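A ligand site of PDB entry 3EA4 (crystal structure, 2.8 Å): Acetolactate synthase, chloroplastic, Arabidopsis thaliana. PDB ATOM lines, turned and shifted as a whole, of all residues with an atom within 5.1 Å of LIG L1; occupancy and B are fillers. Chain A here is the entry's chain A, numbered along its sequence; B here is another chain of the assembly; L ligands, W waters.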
ATOM      1  N   MET A 265      10.021  -8.771   5.257  1.00  0.00           N
ATOM      2  CA  MET A 265       9.171  -9.496   6.200  1.00  0.00           C
ATOM      3  C   MET A 265       8.641  -8.604   7.318  1.00  0.00           C
ATOM      4  O   MET A 265       7.475  -8.675   7.683  1.00  0.00           O
ATOM      5  CB  MET A 265       9.949 -10.683   6.785  1.00  0.00           C
ATOM      6  CG  MET A 265       9.280 -11.388   7.974  1.00  0.00           C
ATOM      7  SD  MET A 265      10.169 -12.851   8.500  1.00  0.00           S
ATOM      8  CE  MET A 265       9.727 -13.998   7.196  1.00  0.00           C
ATOM      9  N   ASP A 290      15.537 -13.866   0.674  1.00  0.00           N
ATOM     10  CA  ASP A 290      14.172 -14.341   0.969  1.00  0.00           C
ATOM     11  C   ASP A 290      13.411 -13.486   1.989  1.00  0.00           C
ATOM     12  O   ASP A 290      12.180 -13.376   1.916  1.00  0.00           O
ATOM     13  CB  ASP A 290      14.183 -15.822   1.391  1.00  0.00           C
ATOM     14  CG  ASP A 290      15.072 -16.082   2.605  1.00  0.00           C
ATOM     15  OD1 ASP A 290      16.266 -16.416   2.421  1.00  0.00           O
ATOM     16  OD2 ASP A 290      14.558 -15.936   3.736  1.00  0.00           O
ATOM     17  N   ARG A 291      14.148 -12.869   2.912  1.00  0.00           N
ATOM     18  CA  ARG A 291      13.565 -11.977   3.905  1.00  0.00           C
ATOM     19  C   ARG A 291      12.844 -10.777   3.301  1.00  0.00           C
ATOM     20  O   ARG A 291      11.892 -10.278   3.873  1.00  0.00           O
ATOM     21  CB  ARG A 291      14.632 -11.491   4.895  1.00  0.00           C
ATOM     22  CG  ARG A 291      14.609 -12.198   6.232  1.00  0.00           C
ATOM     23  CD  ARG A 291      14.525 -13.680   6.029  1.00  0.00           C
ATOM     24  NE  ARG A 291      13.645 -14.300   7.010  1.00  0.00           N
ATOM     25  CZ  ARG A 291      13.110 -15.513   6.878  1.00  0.00           C
ATOM     26  NH1 ARG A 291      13.349 -16.254   5.803  1.00  0.00           N
ATOM     27  NH2 ARG A 291      12.336 -15.987   7.839  1.00  0.00           N
ATOM     28  N   MET A 484      11.731 -13.297  19.568  1.00  0.00           N
ATOM     29  CA  MET A 484      11.437 -13.634  18.176  1.00  0.00           C
ATOM     30  C   MET A 484      10.853 -15.046  18.053  1.00  0.00           C
ATOM     31  O   MET A 484       9.843 -15.254  17.377  1.00  0.00           O
ATOM     32  CB  MET A 484      12.676 -13.479  17.301  1.00  0.00           C
ATOM     33  CG  MET A 484      12.413 -13.542  15.806  1.00  0.00           C
ATOM     34  SD  MET A 484      11.216 -12.288  15.275  1.00  0.00           S
ATOM     35  CE  MET A 484      12.353 -10.983  14.818  1.00  0.00           C
ATOM     36  N   VAL A 485      11.486 -16.010  18.717  1.00  0.00           N
ATOM     37  CA  VAL A 485      11.024 -17.396  18.727  1.00  0.00           C
ATOM     38  C   VAL A 485       9.674 -17.483  19.431  1.00  0.00           C
ATOM     39  O   VAL A 485       8.776 -18.217  18.979  1.00  0.00           O
ATOM     40  CB  VAL A 485      12.054 -18.324  19.404  1.00  0.00           C
ATOM     41  CG1 VAL A 485      11.677 -19.784  19.226  1.00  0.00           C
ATOM     42  CG2 VAL A 485      13.441 -18.075  18.832  1.00  0.00           C
ATOM     43  N   TRP A 488       6.827 -16.403  17.040  1.00  0.00           N
ATOM     44  CA  TRP A 488       6.464 -17.482  16.130  1.00  0.00           C
ATOM     45  C   TRP A 488       5.701 -18.608  16.842  1.00  0.00           C
ATOM     46  O   TRP A 488       4.857 -19.274  16.233  1.00  0.00           O
ATOM     47  CB  TRP A 488       7.712 -18.015  15.416  1.00  0.00           C
ATOM     48  CG  TRP A 488       8.151 -17.174  14.248  1.00  0.00           C
ATOM     49  CD1 TRP A 488       8.522 -15.854  14.277  1.00  0.00           C
ATOM     50  CD2 TRP A 488       8.281 -17.590  12.883  1.00  0.00           C
ATOM     51  NE1 TRP A 488       8.866 -15.423  13.008  1.00  0.00           N
ATOM     52  CE2 TRP A 488       8.724 -16.474  12.136  1.00  0.00           C
ATOM     53  CE3 TRP A 488       8.065 -18.806  12.211  1.00  0.00           C
ATOM     54  CZ2 TRP A 488       8.959 -16.533  10.748  1.00  0.00           C
ATOM     55  CZ3 TRP A 488       8.292 -18.867  10.828  1.00  0.00           C
ATOM     56  CH2 TRP A 488       8.731 -17.743  10.118  1.00  0.00           C
ATOM     57  N   SER A 567       6.886 -16.466   5.993  1.00  0.00           N
ATOM     58  CA  SER A 567       7.924 -16.951   5.077  1.00  0.00           C
ATOM     59  C   SER A 567       7.355 -17.553   3.808  1.00  0.00           C
ATOM     60  O   SER A 567       6.457 -18.401   3.853  1.00  0.00           O
ATOM     61  CB  SER A 567       8.812 -17.981   5.773  1.00  0.00           C
ATOM     62  OG  SER A 567       9.856 -17.343   6.480  1.00  0.00           O
ATOM     63  N   GLY B  35      14.866 -20.490  14.753  1.00  0.00           N
ATOM     64  CA  GLY B  35      13.914 -20.614  13.659  1.00  0.00           C
ATOM     65  C   GLY B  35      13.894 -21.978  13.004  1.00  0.00           C
ATOM     66  O   GLY B  35      12.826 -22.583  12.862  1.00  0.00           O
ATOM     67  N   ALA B  36      15.068 -22.469  12.620  1.00  0.00           N
ATOM     68  CA  ALA B  36      15.174 -23.707  11.856  1.00  0.00           C
ATOM     69  C   ALA B  36      14.977 -24.977  12.679  1.00  0.00           C
ATOM     70  O   ALA B  36      14.953 -26.078  12.116  1.00  0.00           O
ATOM     71  CB  ALA B  36      16.490 -23.758  11.112  1.00  0.00           C
ATOM     72  N   MET B  38      12.624 -24.953  15.566  1.00  0.00           N
ATOM     73  CA  MET B  38      11.412 -24.783  16.374  1.00  0.00           C
ATOM     74  C   MET B  38      10.574 -26.047  16.471  1.00  0.00           C
ATOM     75  O   MET B  38      10.106 -26.402  17.552  1.00  0.00           O
ATOM     76  CB  MET B  38      10.551 -23.638  15.830  1.00  0.00           C
ATOM     77  CG  MET B  38      11.075 -22.271  16.189  1.00  0.00           C
ATOM     78  SD  MET B  38       9.878 -20.998  15.783  1.00  0.00           S
ATOM     79  CE  MET B  38       8.718 -21.172  17.150  1.00  0.00           C
ATOM     80  N   SER B  82      19.757 -23.578  12.783  1.00  0.00           N
ATOM     81  CA  SER B  82      20.640 -23.429  11.639  1.00  0.00           C
ATOM     82  C   SER B  82      21.578 -22.244  11.827  1.00  0.00           C
ATOM     83  O   SER B  82      21.472 -21.510  12.820  1.00  0.00           O
ATOM     84  CB  SER B  82      19.819 -23.228  10.372  1.00  0.00           C
ATOM     85  OG  SER B  82      19.263 -21.932  10.334  1.00  0.00           O
ATOM     86  N   VAL B 110      17.940 -24.913   6.925  1.00  0.00           N
ATOM     87  CA  VAL B 110      16.905 -24.292   6.102  1.00  0.00           C
ATOM     88  C   VAL B 110      16.181 -25.350   5.242  1.00  0.00           C
ATOM     89  O   VAL B 110      16.708 -26.452   5.045  1.00  0.00           O
ATOM     90  CB  VAL B 110      17.470 -23.148   5.214  1.00  0.00           C
ATOM     91  CG1 VAL B 110      18.135 -22.087   6.077  1.00  0.00           C
ATOM     92  CG2 VAL B 110      18.460 -23.683   4.177  1.00  0.00           C
ATOM     93  N   PRO B 111      14.977 -25.034   4.716  1.00  0.00           N
ATOM     94  CA  PRO B 111      14.318 -25.997   3.827  1.00  0.00           C
ATOM     95  C   PRO B 111      15.228 -26.460   2.692  1.00  0.00           C
ATOM     96  O   PRO B 111      16.022 -25.668   2.177  1.00  0.00           O
ATOM     97  CB  PRO B 111      13.128 -25.203   3.280  1.00  0.00           C
ATOM     98  CG  PRO B 111      12.831 -24.206   4.314  1.00  0.00           C
ATOM     99  CD  PRO B 111      14.169 -23.816   4.900  1.00  0.00           C
ATOM    100  N   MET B 114      16.013 -24.325  -0.264  1.00  0.00           N
ATOM    101  CA  MET B 114      16.752 -23.090   0.032  1.00  0.00           C
ATOM    102  C   MET B 114      18.251 -23.332   0.111  1.00  0.00           C
ATOM    103  O   MET B 114      19.026 -22.369   0.111  1.00  0.00           O
ATOM    104  CB  MET B 114      16.280 -22.455   1.349  1.00  0.00           C
ATOM    105  CG  MET B 114      14.813 -22.085   1.438  1.00  0.00           C
ATOM    106  SD  MET B 114      14.267 -20.893   0.192  1.00  0.00           S
ATOM    107  CE  MET B 114      15.326 -19.480   0.520  1.00  0.00           C
ATOM    108  N   ALA B 119      20.583 -18.571   1.889  1.00  0.00           N
ATOM    109  CA  ALA B 119      19.330 -18.303   2.575  1.00  0.00           C
ATOM    110  C   ALA B 119      19.554 -17.740   3.974  1.00  0.00           C
ATOM    111  O   ALA B 119      20.674 -17.791   4.518  1.00  0.00           O
ATOM    112  CB  ALA B 119      18.482 -19.572   2.636  1.00  0.00           C
ATOM    113  N   PHE B 120      18.491 -17.196   4.541  1.00  0.00           N
ATOM    114  CA  PHE B 120      18.486 -16.683   5.897  1.00  0.00           C
ATOM    115  C   PHE B 120      18.950 -17.745   6.889  1.00  0.00           C
ATOM    116  O   PHE B 120      18.365 -18.830   6.967  1.00  0.00           O
ATOM    117  CB  PHE B 120      17.078 -16.194   6.252  1.00  0.00           C
ATOM    118  CG  PHE B 120      16.945 -15.643   7.631  1.00  0.00           C
ATOM    119  CD1 PHE B 120      17.680 -14.525   8.027  1.00  0.00           C
ATOM    120  CD2 PHE B 120      16.072 -16.223   8.542  1.00  0.00           C
ATOM    121  CE1 PHE B 120      17.552 -14.002   9.303  1.00  0.00           C
ATOM    122  CE2 PHE B 120      15.932 -15.712   9.833  1.00  0.00           C
ATOM    123  CZ  PHE B 120      16.673 -14.598  10.217  1.00  0.00           C
ATOM    124  N   GLN B 121      20.002 -17.422   7.626  1.00  0.00           N
ATOM    125  CA  GLN B 121      20.597 -18.310   8.633  1.00  0.00           C
ATOM    126  C   GLN B 121      21.043 -19.651   8.063  1.00  0.00           C
ATOM    127  O   GLN B 121      20.887 -20.698   8.699  1.00  0.00           O
ATOM    128  CB  GLN B 121      19.647 -18.522   9.817  1.00  0.00           C
ATOM    129  CG  GLN B 121      19.140 -17.225  10.407  1.00  0.00           C
ATOM    130  CD  GLN B 121      18.672 -17.397  11.843  1.00  0.00           C
ATOM    131  OE1 GLN B 121      17.771 -18.191  12.124  1.00  0.00           O
ATOM    132  NE2 GLN B 121      19.281 -16.636  12.758  1.00  0.00           N
ATOM    133  N   LYS B 170      14.298 -27.899   7.580  1.00  0.00           N
ATOM    134  CA  LYS B 170      13.047 -27.540   8.233  1.00  0.00           C
ATOM    135  C   LYS B 170      11.816 -28.195   7.607  1.00  0.00           C
ATOM    136  O   LYS B 170      10.878 -28.578   8.322  1.00  0.00           O
ATOM    137  CB  LYS B 170      12.873 -26.021   8.247  1.00  0.00           C
ATOM    138  CG  LYS B 170      11.962 -25.541   9.367  1.00  0.00           C
ATOM    139  CD  LYS B 170      11.474 -24.117   9.182  1.00  0.00           C
ATOM    140  CE  LYS B 170      10.501 -23.764  10.304  1.00  0.00           C
ATOM    141  NZ  LYS B 170       9.778 -22.472  10.128  1.00  0.00           N
HETATM  142  C1  LIG L   1      15.713 -19.718   9.592  1.00  0.00           C
HETATM  143  O1  LIG L   1      15.767 -20.723   8.550  1.00  0.00           O
HETATM  144  C2  LIG L   1      14.539 -20.808   8.003  1.00  0.00           C
HETATM  145  O2  LIG L   1      13.681 -21.320   8.715  1.00  0.00           O
HETATM  146  C3  LIG L   1      14.238 -20.266   6.597  1.00  0.00           C
HETATM  147  C4  LIG L   1      15.277 -19.688   5.858  1.00  0.00           C
HETATM  148  C5  LIG L   1      15.059 -19.191   4.565  1.00  0.00           C
HETATM  149  C6  LIG L   1      13.787 -19.252   3.997  1.00  0.00           C
HETATM  150  C7  LIG L   1      12.733 -19.809   4.721  1.00  0.00           C
HETATM  151  C8  LIG L   1      12.964 -20.311   6.014  1.00  0.00           C
HETATM  152  S1  LIG L   1      11.530 -20.986   6.813  1.00  0.00           S
HETATM  153  O3  LIG L   1      11.461 -22.406   6.603  1.00  0.00           O
HETATM  154  O4  LIG L   1      10.324 -20.341   6.213  1.00  0.00           O
HETATM  155  N1  LIG L   1      11.445 -20.701   8.447  1.00  0.00           N
HETATM  156  C9  LIG L   1      11.693 -19.476   8.940  1.00  0.00           C
HETATM  157  O5  LIG L   1      11.973 -18.501   8.258  1.00  0.00           O
HETATM  158  N2  LIG L   1      11.629 -19.380  10.290  1.00  0.00           N
HETATM  159  C10 LIG L   1      11.843 -18.275  11.026  1.00  0.00           C
HETATM  160  N3  LIG L   1      11.718 -18.369  12.409  1.00  0.00           N
HETATM  161  C11 LIG L   1      11.931 -17.245  13.213  1.00  0.00           C
HETATM  162  C12 LIG L   1      11.786 -17.398  14.731  1.00  0.00           C
HETATM  163  C13 LIG L   1      12.294 -15.875  12.623  1.00  0.00           C
HETATM  164  C14 LIG L   1      12.393 -15.893  11.228  1.00  0.00           C
HETATM  165  N4  LIG L   1      12.165 -17.039  10.450  1.00  0.00           N
HETATM  166  O1  LG2 L   2      16.036 -11.796  24.059  1.00  0.00           O
HETATM  167  P1  LG2 L   2      16.622 -11.882  22.701  1.00  0.00           P
HETATM  168  O2  LG2 L   2      18.163 -11.526  22.760  1.00  0.00           O
HETATM  169  O3  LG2 L   2      16.002 -10.835  21.664  1.00  0.00           O
HETATM  170  P2  LG2 L   2      14.441 -10.556  21.501  1.00  0.00           P
HETATM  171  O4  LG2 L   2      14.207  -9.114  21.267  1.00  0.00           O
HETATM  172  O5  LG2 L   2      13.917 -11.450  20.255  1.00  0.00           O
HETATM  173  O6  LG2 L   2      13.661 -11.088  22.821  1.00  0.00           O
HETATM  174  O7  LG2 L   2      16.481 -13.328  22.011  1.00  0.00           O
HETATM  175  C1  LG2 L   2      16.658 -13.570  20.604  1.00  0.00           C
HETATM  176  C2  LG2 L   2      15.717 -14.696  20.202  1.00  0.00           C
HETATM  177  C3  LG2 L   2      16.151 -15.456  18.947  1.00  0.00           C
HETATM  178  S1  LG2 L   2      15.779 -14.840  17.379  1.00  0.00           S
HETATM  179  C4  LG2 L   2      16.484 -16.147  16.499  1.00  0.00           C
HETATM  180  C5  LG2 L   2      16.517 -16.266  15.168  1.00  0.00           C
HETATM  181  C6  LG2 L   2      15.897 -15.200  14.256  1.00  0.00           C
HETATM  182  O8  LG2 L   2      17.199 -17.514  14.512  1.00  0.00           O
HETATM  183  N1  LG2 L   2      17.048 -17.120  17.556  1.00  0.00           N
HETATM  184  C7  LG2 L   2      16.832 -16.692  18.825  1.00  0.00           C
HETATM  185  C8  LG2 L   2      17.289 -17.485  20.061  1.00  0.00           C
HETATM  186  C9  LG2 L   2      17.766 -18.376  17.210  1.00  0.00           C
HETATM  187  C10 LG2 L   2      19.303 -18.159  17.376  1.00  0.00           C
HETATM  188  C11 LG2 L   2      20.073 -17.182  16.707  1.00  0.00           C
HETATM  189  N2  LG2 L   2      19.536 -16.345  15.829  1.00  0.00           N
HETATM  190  N3  LG2 L   2      21.398 -17.094  16.943  1.00  0.00           N
HETATM  191  C12 LG2 L   2      22.003 -17.911  17.820  1.00  0.00           C
HETATM  192  C13 LG2 L   2      23.508 -17.761  18.062  1.00  0.00           C
HETATM  193  N4  LG2 L   2      21.299 -18.852  18.475  1.00  0.00           N
HETATM  194  C14 LG2 L   2      19.987 -18.987  18.279  1.00  0.00           C
HETATM  195  O   HOH W   1       9.491 -24.747   5.169  1.00  0.00           O
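The guanidinium group (NH2) of Arg 291 sits at hydrogen-bond distance from an oxygen (O5) of LIG L1, at 2.6 Å.
An oxygen (O5) of LIG L1 sits at hydrogen-bond distance from the side-chain hydroxyl (OG) of Ser 567, 3.0 Å away.
The side-chain amino group (NZ) of Lys 170 of chain B sits at hydrogen-bond distance from a nitrogen (N1) of LIG L1.
The side-chain amide oxygen (OE1) of Gln 121 of chain B lies within hydrogen-bond range of an oxygen (O8) of LG2 L2 (2.5 Å).
The backbone NH (N) of Met 484 sits at hydrogen-bond distance from an oxygen (O5) of LG2 L2.
The guanidinium group (NH2) of Arg 291 lies within hydrogen-bond range of the side-chain hydroxyl (OG) of Ser 567.
NH1 of Arg 291 is in salt-bridge range of OD2 of Asp 290, at 2.4 Å.
N of Met 265 is in hydrogen-bond range of O of Arg 291 (2.8 Å).
The side-chain carboxylate (OD1) of Asp 290 is in hydrogen-bond range of the backbone NH (N) of Phe 120 of chain B (3.2 Å).
The side-chain hydroxyl (OG) of Ser 82 of chain B sits at hydrogen-bond distance from the backbone carbonyl oxygen (O) of Gln 121 of chain B (2.6 Å).
Asp 290 touches LIG L1 (OD2 to C5, 3.4 Å).
O of Met 484 touches C12 of LIG L1, at 3.9 Å.
Trp 488 touches LIG L1.
CA of Gly 35 of chain B touches N3 of LIG L1 (3.4 Å).
Val 110 of chain B touches LIG L1.
Pro 111 of chain B touches LIG L1.
Met 114 of chain B touches LIG L1.
Ala 119 of chain B touches LIG L1 (CB to C5, 3.9 Å).
Phe 120 of chain B touches LIG L1.
OE1 of Gln 121 of chain B touches C1 of LIG L1, at 3.6 Å.
Hydrophobic or aromatic side chains that line LIG L1: Met 484, Trp 488, Val 110 of chain B, Pro 111 of chain B, Met 114 of chain B, Ala 119 of chain B and Phe 120 of chain B.
The nearest printed residue that does not touch LIG L1 is Ala 36 of chain B (4.04 Å).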
